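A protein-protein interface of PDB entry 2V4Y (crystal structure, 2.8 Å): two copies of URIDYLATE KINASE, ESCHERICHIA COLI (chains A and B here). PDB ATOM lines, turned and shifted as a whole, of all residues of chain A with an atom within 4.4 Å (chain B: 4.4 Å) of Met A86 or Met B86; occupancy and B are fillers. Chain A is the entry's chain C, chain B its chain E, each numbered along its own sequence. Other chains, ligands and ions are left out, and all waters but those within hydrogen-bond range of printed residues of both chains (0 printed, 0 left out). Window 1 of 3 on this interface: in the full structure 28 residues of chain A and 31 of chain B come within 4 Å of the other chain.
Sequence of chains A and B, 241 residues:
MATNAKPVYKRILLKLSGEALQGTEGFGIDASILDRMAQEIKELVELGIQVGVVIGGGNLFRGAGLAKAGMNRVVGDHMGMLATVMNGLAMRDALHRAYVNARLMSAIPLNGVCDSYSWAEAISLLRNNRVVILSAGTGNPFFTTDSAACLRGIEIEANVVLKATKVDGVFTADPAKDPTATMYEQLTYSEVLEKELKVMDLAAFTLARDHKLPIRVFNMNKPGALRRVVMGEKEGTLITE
SD of Met A79 sits close to O of Met B86 (3.7 Å). The side-chain sulfur (SD) of Met B79 sits close to the backbone carbonyl oxygen (O) of Met A86 (3.8 Å).
Among the printed residues, pairs that only touch across the chains: Leu A60 with Leu B60, Phe A61 with Met B86, Met A79 with Leu B89, Met A79 with Ala B90, Leu A82 with Val B85, Leu A82 with Met B86, Leu A82 with Leu B89, Val A85 with Leu B82, Met A86 with Phe B61, Met A86 with Leu B82, Met A86 with Met B86, Leu A89 with Met B79 and Ala A90 with Met B79.
Printed residues of chain B within 4 Å of Leu A60: Leu B60 (3.2 Å). Printed residues of chain B within 4 Å of Val A85: Leu B82. Of the printed residues of chain B, Met A86 touches Phe B61 (3.6 Å), Met B79 (3.3 Å), Leu B82 (3.8 Å) and Met B86 (3.8 Å). Printed residues of chain B within 4 Å of Ala A90: Met B79 (3.9 Å). Of the printed residues of chain A, Phe B61 touches Met A86. Of the printed residues of chain A, Met B86 touches Phe A61 (3.6 Å), Met A79 (3.2 Å), Leu A82 (3.8 Å) and Met A86 (3.8 Å).
Hydrophobic or aromatic side chains of chain B that line the printed part of chain A: Leu B60, Phe B61, Met B79, Leu B82, Val B85, Met B86, Leu B89 and Ala B90. Among the printed residues, 15 pairs touch across the chains.
Phe A61 touches Met B86, and with the chains exchanged Met A86 touches Phe B61. Leu A82 touches Met B86, and with the chains exchanged Met A86 touches Leu B82. Leu A82 touches Leu B89, but with the chains exchanged Leu A89 does not touch Leu B82 (4.001 Å). Met B86 touches its own counterpart, Met A86.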
ATOM      1  N   LEU A  60       2.561  -3.321 -21.434  1.00  0.00           N
ATOM      2  CA  LEU A  60       2.945  -4.127 -22.587  1.00  0.00           C
ATOM      3  C   LEU A  60       3.235  -3.267 -23.807  1.00  0.00           C
ATOM      4  O   LEU A  60       3.942  -3.687 -24.722  1.00  0.00           O
ATOM      5  CB  LEU A  60       1.859  -5.152 -22.904  1.00  0.00           C
ATOM      6  CG  LEU A  60       1.887  -6.392 -22.006  1.00  0.00           C
ATOM      7  CD1 LEU A  60       0.651  -7.262 -22.235  1.00  0.00           C
ATOM      8  CD2 LEU A  60       3.167  -7.181 -22.235  1.00  0.00           C
ATOM      9  N   PHE A  61       2.691  -2.058 -23.819  1.00  0.00           N
ATOM     10  CA  PHE A  61       2.975  -1.131 -24.896  1.00  0.00           C
ATOM     11  C   PHE A  61       3.166   0.301 -24.409  1.00  0.00           C
ATOM     12  O   PHE A  61       2.224   0.951 -23.945  1.00  0.00           O
ATOM     13  CB  PHE A  61       1.878  -1.179 -25.956  1.00  0.00           C
ATOM     14  CG  PHE A  61       2.074  -0.181 -27.061  1.00  0.00           C
ATOM     15  CD1 PHE A  61       3.076  -0.364 -28.003  1.00  0.00           C
ATOM     16  CD2 PHE A  61       1.270   0.952 -27.142  1.00  0.00           C
ATOM     17  CE1 PHE A  61       3.264   0.549 -29.003  1.00  0.00           C
ATOM     18  CE2 PHE A  61       1.454   1.876 -28.143  1.00  0.00           C
ATOM     19  CZ  PHE A  61       2.453   1.675 -29.080  1.00  0.00           C
ATOM     20  N   MET A  79      -2.259  -0.658 -31.200  1.00  0.00           N
ATOM     21  CA  MET A  79      -1.285  -1.538 -30.570  1.00  0.00           C
ATOM     22  C   MET A  79      -1.600  -1.645 -29.089  1.00  0.00           C
ATOM     23  O   MET A  79      -1.556  -2.732 -28.508  1.00  0.00           O
ATOM     24  CB  MET A  79       0.129  -1.021 -30.784  1.00  0.00           C
ATOM     25  CG  MET A  79       0.602  -1.123 -32.211  1.00  0.00           C
ATOM     26  SD  MET A  79       2.314  -0.647 -32.376  1.00  0.00           S
ATOM     27  CE  MET A  79       3.130  -1.870 -31.369  1.00  0.00           C
ATOM     28  N   LEU A  82      -4.645  -3.855 -28.510  1.00  0.00           N
ATOM     29  CA  LEU A  82      -4.267  -5.259 -28.479  1.00  0.00           C
ATOM     30  C   LEU A  82      -3.583  -5.589 -27.167  1.00  0.00           C
ATOM     31  O   LEU A  82      -3.800  -6.657 -26.590  1.00  0.00           O
ATOM     32  CB  LEU A  82      -3.356  -5.608 -29.651  1.00  0.00           C
ATOM     33  CG  LEU A  82      -3.984  -5.465 -31.036  1.00  0.00           C
ATOM     34  CD1 LEU A  82      -3.069  -6.059 -32.076  1.00  0.00           C
ATOM     35  CD2 LEU A  82      -5.351  -6.122 -31.099  1.00  0.00           C
ATOM     36  N   ALA A  83      -2.758  -4.659 -26.697  1.00  0.00           N
ATOM     37  CA  ALA A  83      -2.047  -4.836 -25.439  1.00  0.00           C
ATOM     38  C   ALA A  83      -3.015  -5.139 -24.293  1.00  0.00           C
ATOM     39  O   ALA A  83      -2.790  -6.052 -23.491  1.00  0.00           O
ATOM     40  CB  ALA A  83      -1.219  -3.604 -25.130  1.00  0.00           C
ATOM     41  N   THR A  84      -4.094  -4.366 -24.225  1.00  0.00           N
ATOM     42  CA  THR A  84      -5.092  -4.559 -23.191  1.00  0.00           C
ATOM     43  C   THR A  84      -5.709  -5.951 -23.239  1.00  0.00           C
ATOM     44  O   THR A  84      -6.137  -6.471 -22.218  1.00  0.00           O
ATOM     45  CB  THR A  84      -6.224  -3.512 -23.288  1.00  0.00           C
ATOM     46  OG1 THR A  84      -7.099  -3.838 -24.373  1.00  0.00           O
ATOM     47  CG2 THR A  84      -5.657  -2.142 -23.503  1.00  0.00           C
ATOM     48  N   VAL A  85      -5.771  -6.546 -24.424  1.00  0.00           N
ATOM     49  CA  VAL A  85      -6.361  -7.865 -24.556  1.00  0.00           C
ATOM     50  C   VAL A  85      -5.405  -8.917 -24.039  1.00  0.00           C
ATOM     51  O   VAL A  85      -5.829  -9.940 -23.531  1.00  0.00           O
ATOM     52  CB  VAL A  85      -6.762  -8.193 -25.998  1.00  0.00           C
ATOM     53  CG1 VAL A  85      -7.415  -9.543 -26.055  1.00  0.00           C
ATOM     54  CG2 VAL A  85      -7.712  -7.122 -26.553  1.00  0.00           C
ATOM     55  N   MET A  86      -4.110  -8.668 -24.161  1.00  0.00           N
ATOM     56  CA  MET A  86      -3.128  -9.594 -23.616  1.00  0.00           C
ATOM     57  C   MET A  86      -3.226  -9.602 -22.102  1.00  0.00           C
ATOM     58  O   MET A  86      -3.204 -10.656 -21.479  1.00  0.00           O
ATOM     59  CB  MET A  86      -1.719  -9.211 -24.057  1.00  0.00           C
ATOM     60  CG  MET A  86      -1.481  -9.374 -25.543  1.00  0.00           C
ATOM     61  SD  MET A  86       0.091  -8.673 -26.057  1.00  0.00           S
ATOM     62  CE  MET A  86       1.215  -9.776 -25.199  1.00  0.00           C
ATOM     63  N   ASN A  87      -3.349  -8.417 -21.516  1.00  0.00           N
ATOM     64  CA  ASN A  87      -3.550  -8.281 -20.080  1.00  0.00           C
ATOM     65  C   ASN A  87      -4.828  -8.959 -19.622  1.00  0.00           C
ATOM     66  O   ASN A  87      -4.814  -9.731 -18.676  1.00  0.00           O
ATOM     67  CB  ASN A  87      -3.561  -6.810 -19.667  1.00  0.00           C
ATOM     68  CG  ASN A  87      -2.161  -6.225 -19.545  1.00  0.00           C
ATOM     69  OD1 ASN A  87      -1.187  -6.947 -19.347  1.00  0.00           O
ATOM     70  ND2 ASN A  87      -2.061  -4.911 -19.659  1.00  0.00           N
ATOM     71  N   GLY A  88      -5.933  -8.680 -20.300  1.00  0.00           N
ATOM     72  CA  GLY A  88      -7.198  -9.344 -20.010  1.00  0.00           C
ATOM     73  C   GLY A  88      -7.083 -10.861 -20.099  1.00  0.00           C
ATOM     74  O   GLY A  88      -7.585 -11.603 -19.259  1.00  0.00           O
ATOM     75  N   LEU A  89      -6.398 -11.318 -21.136  1.00  0.00           N
ATOM     76  CA  LEU A  89      -6.178 -12.734 -21.376  1.00  0.00           C
ATOM     77  C   LEU A  89      -5.468 -13.339 -20.167  1.00  0.00           C
ATOM     78  O   LEU A  89      -5.868 -14.387 -19.656  1.00  0.00           O
ATOM     79  CB  LEU A  89      -5.306 -12.889 -22.622  1.00  0.00           C
ATOM     80  CG  LEU A  89      -5.681 -13.886 -23.708  1.00  0.00           C
ATOM     81  CD1 LEU A  89      -7.168 -14.114 -23.731  1.00  0.00           C
ATOM     82  CD2 LEU A  89      -5.187 -13.366 -25.050  1.00  0.00           C
ATOM     83  N   ALA A  90      -4.408 -12.671 -19.714  1.00  0.00           N
ATOM     84  CA  ALA A  90      -3.620 -13.124 -18.569  1.00  0.00           C
ATOM     85  C   ALA A  90      -4.448 -13.117 -17.285  1.00  0.00           C
ATOM     86  O   ALA A  90      -4.329 -14.018 -16.456  1.00  0.00           O
ATOM     87  CB  ALA A  90      -2.399 -12.252 -18.406  1.00  0.00           C
ATOM     88  N   LEU B  60       7.556  -8.594 -27.134  1.00  0.00           N
ATOM     89  CA  LEU B  60       6.408  -8.001 -26.459  1.00  0.00           C
ATOM     90  C   LEU B  60       5.783  -8.960 -25.469  1.00  0.00           C
ATOM     91  O   LEU B  60       5.076  -8.547 -24.561  1.00  0.00           O
ATOM     92  CB  LEU B  60       5.362  -7.540 -27.473  1.00  0.00           C
ATOM     93  CG  LEU B  60       5.681  -6.202 -28.134  1.00  0.00           C
ATOM     94  CD1 LEU B  60       4.725  -5.912 -29.282  1.00  0.00           C
ATOM     95  CD2 LEU B  60       5.640  -5.091 -27.102  1.00  0.00           C
ATOM     96  N   PHE B  61       6.041 -10.246 -25.645  1.00  0.00           N
ATOM     97  CA  PHE B  61       5.521 -11.235 -24.716  1.00  0.00           C
ATOM     98  C   PHE B  61       6.510 -12.360 -24.455  1.00  0.00           C
ATOM     99  O   PHE B  61       6.789 -13.171 -25.339  1.00  0.00           O
ATOM    100  CB  PHE B  61       4.194 -11.819 -25.206  1.00  0.00           C
ATOM    101  CG  PHE B  61       3.665 -12.913 -24.321  1.00  0.00           C
ATOM    102  CD1 PHE B  61       3.104 -12.612 -23.084  1.00  0.00           C
ATOM    103  CD2 PHE B  61       3.755 -14.242 -24.711  1.00  0.00           C
ATOM    104  CE1 PHE B  61       2.630 -13.611 -22.262  1.00  0.00           C
ATOM    105  CE2 PHE B  61       3.280 -15.245 -23.896  1.00  0.00           C
ATOM    106  CZ  PHE B  61       2.716 -14.928 -22.666  1.00  0.00           C
ATOM    107  N   MET B  79      -1.635 -14.979 -26.312  1.00  0.00           N
ATOM    108  CA  MET B  79      -1.048 -13.703 -25.943  1.00  0.00           C
ATOM    109  C   MET B  79       0.071 -13.375 -26.919  1.00  0.00           C
ATOM    110  O   MET B  79       0.163 -12.249 -27.414  1.00  0.00           O
ATOM    111  CB  MET B  79      -0.540 -13.745 -24.505  1.00  0.00           C
ATOM    112  CG  MET B  79      -1.649 -13.811 -23.474  1.00  0.00           C
ATOM    113  SD  MET B  79      -1.035 -13.706 -21.795  1.00  0.00           S
ATOM    114  CE  MET B  79      -0.276 -12.073 -21.826  1.00  0.00           C
ATOM    115  N   LEU B  82      -1.313 -12.290 -30.275  1.00  0.00           N
ATOM    116  CA  LEU B  82      -1.660 -10.876 -30.307  1.00  0.00           C
ATOM    117  C   LEU B  82      -0.393 -10.048 -30.377  1.00  0.00           C
ATOM    118  O   LEU B  82      -0.351  -9.033 -31.063  1.00  0.00           O
ATOM    119  CB  LEU B  82      -2.479 -10.484 -29.084  1.00  0.00           C
ATOM    120  CG  LEU B  82      -3.834 -11.166 -28.965  1.00  0.00           C
ATOM    121  CD1 LEU B  82      -4.636 -10.550 -27.838  1.00  0.00           C
ATOM    122  CD2 LEU B  82      -4.591 -11.060 -30.270  1.00  0.00           C
ATOM    123  N   ALA B  83       0.641 -10.488 -29.669  1.00  0.00           N
ATOM    124  CA  ALA B  83       1.901  -9.764 -29.650  1.00  0.00           C
ATOM    125  C   ALA B  83       2.432  -9.575 -31.063  1.00  0.00           C
ATOM    126  O   ALA B  83       2.897  -8.498 -31.428  1.00  0.00           O
ATOM    127  CB  ALA B  83       2.916 -10.492 -28.796  1.00  0.00           C
ATOM    128  N   THR B  84       2.355 -10.624 -31.866  1.00  0.00           N
ATOM    129  CA  THR B  84       2.868 -10.563 -33.223  1.00  0.00           C
ATOM    130  C   THR B  84       2.111  -9.528 -34.034  1.00  0.00           C
ATOM    131  O   THR B  84       2.657  -8.961 -34.975  1.00  0.00           O
ATOM    132  CB  THR B  84       2.753 -11.919 -33.932  1.00  0.00           C
ATOM    133  OG1 THR B  84       1.381 -12.178 -34.276  1.00  0.00           O
ATOM    134  CG2 THR B  84       3.289 -13.030 -33.044  1.00  0.00           C
ATOM    135  N   VAL B  85       0.853  -9.285 -33.685  1.00  0.00           N
ATOM    136  CA  VAL B  85       0.041  -8.341 -34.440  1.00  0.00           C
ATOM    137  C   VAL B  85       0.457  -6.926 -34.095  1.00  0.00           C
ATOM    138  O   VAL B  85       0.386  -6.031 -34.921  1.00  0.00           O
ATOM    139  CB  VAL B  85      -1.488  -8.525 -34.192  1.00  0.00           C
ATOM    140  CG1 VAL B  85      -2.288  -7.584 -35.073  1.00  0.00           C
ATOM    141  CG2 VAL B  85      -1.916  -9.976 -34.435  1.00  0.00           C
ATOM    142  N   MET B  86       0.897  -6.728 -32.861  1.00  0.00           N
ATOM    143  CA  MET B  86       1.391  -5.423 -32.454  1.00  0.00           C
ATOM    144  C   MET B  86       2.662  -5.105 -33.226  1.00  0.00           C
ATOM    145  O   MET B  86       2.811  -4.006 -33.764  1.00  0.00           O
ATOM    146  CB  MET B  86       1.641  -5.382 -30.951  1.00  0.00           C
ATOM    147  CG  MET B  86       0.370  -5.505 -30.119  1.00  0.00           C
ATOM    148  SD  MET B  86       0.740  -5.704 -28.375  1.00  0.00           S
ATOM    149  CE  MET B  86       1.488  -4.093 -28.055  1.00  0.00           C
ATOM    150  N   ASN B  87       3.569  -6.077 -33.290  1.00  0.00           N
ATOM    151  CA  ASN B  87       4.772  -5.945 -34.106  1.00  0.00           C
ATOM    152  C   ASN B  87       4.469  -5.653 -35.574  1.00  0.00           C
ATOM    153  O   ASN B  87       5.029  -4.723 -36.150  1.00  0.00           O
ATOM    154  CB  ASN B  87       5.640  -7.188 -33.991  1.00  0.00           C
ATOM    155  CG  ASN B  87       6.450  -7.213 -32.722  1.00  0.00           C
ATOM    156  OD1 ASN B  87       6.716  -6.175 -32.126  1.00  0.00           O
ATOM    157  ND2 ASN B  87       6.861  -8.405 -32.304  1.00  0.00           N
ATOM    158  N   GLY B  88       3.584  -6.451 -36.172  1.00  0.00           N
ATOM    159  CA  GLY B  88       3.159  -6.230 -37.539  1.00  0.00           C
ATOM    160  C   GLY B  88       2.565  -4.850 -37.722  1.00  0.00           C
ATOM    161  O   GLY B  88       2.823  -4.161 -38.707  1.00  0.00           O
ATOM    162  N   LEU B  89       1.758  -4.444 -36.754  1.00  0.00           N
ATOM    163  CA  LEU B  89       1.114  -3.144 -36.771  1.00  0.00           C
ATOM    164  C   LEU B  89       2.182  -2.050 -36.840  1.00  0.00           C
ATOM    165  O   LEU B  89       2.085  -1.111 -37.624  1.00  0.00           O
ATOM    166  CB  LEU B  89       0.266  -3.002 -35.501  1.00  0.00           C
ATOM    167  CG  LEU B  89      -1.160  -2.459 -35.545  1.00  0.00           C
ATOM    168  CD1 LEU B  89      -1.838  -2.754 -36.869  1.00  0.00           C
ATOM    169  CD2 LEU B  89      -1.946  -3.058 -34.398  1.00  0.00           C
ATOM    170  N   ALA B  90       3.212  -2.197 -36.013  1.00  0.00           N
ATOM    171  CA  ALA B  90       4.308  -1.236 -35.944  1.00  0.00           C
ATOM    172  C   ALA B  90       5.113  -1.221 -37.229  1.00  0.00           C
ATOM    173  O   ALA B  90       5.539  -0.169 -37.695  1.00  0.00           O
ATOM    174  CB  ALA B  90       5.222  -1.559 -34.761  1.00  0.00           C
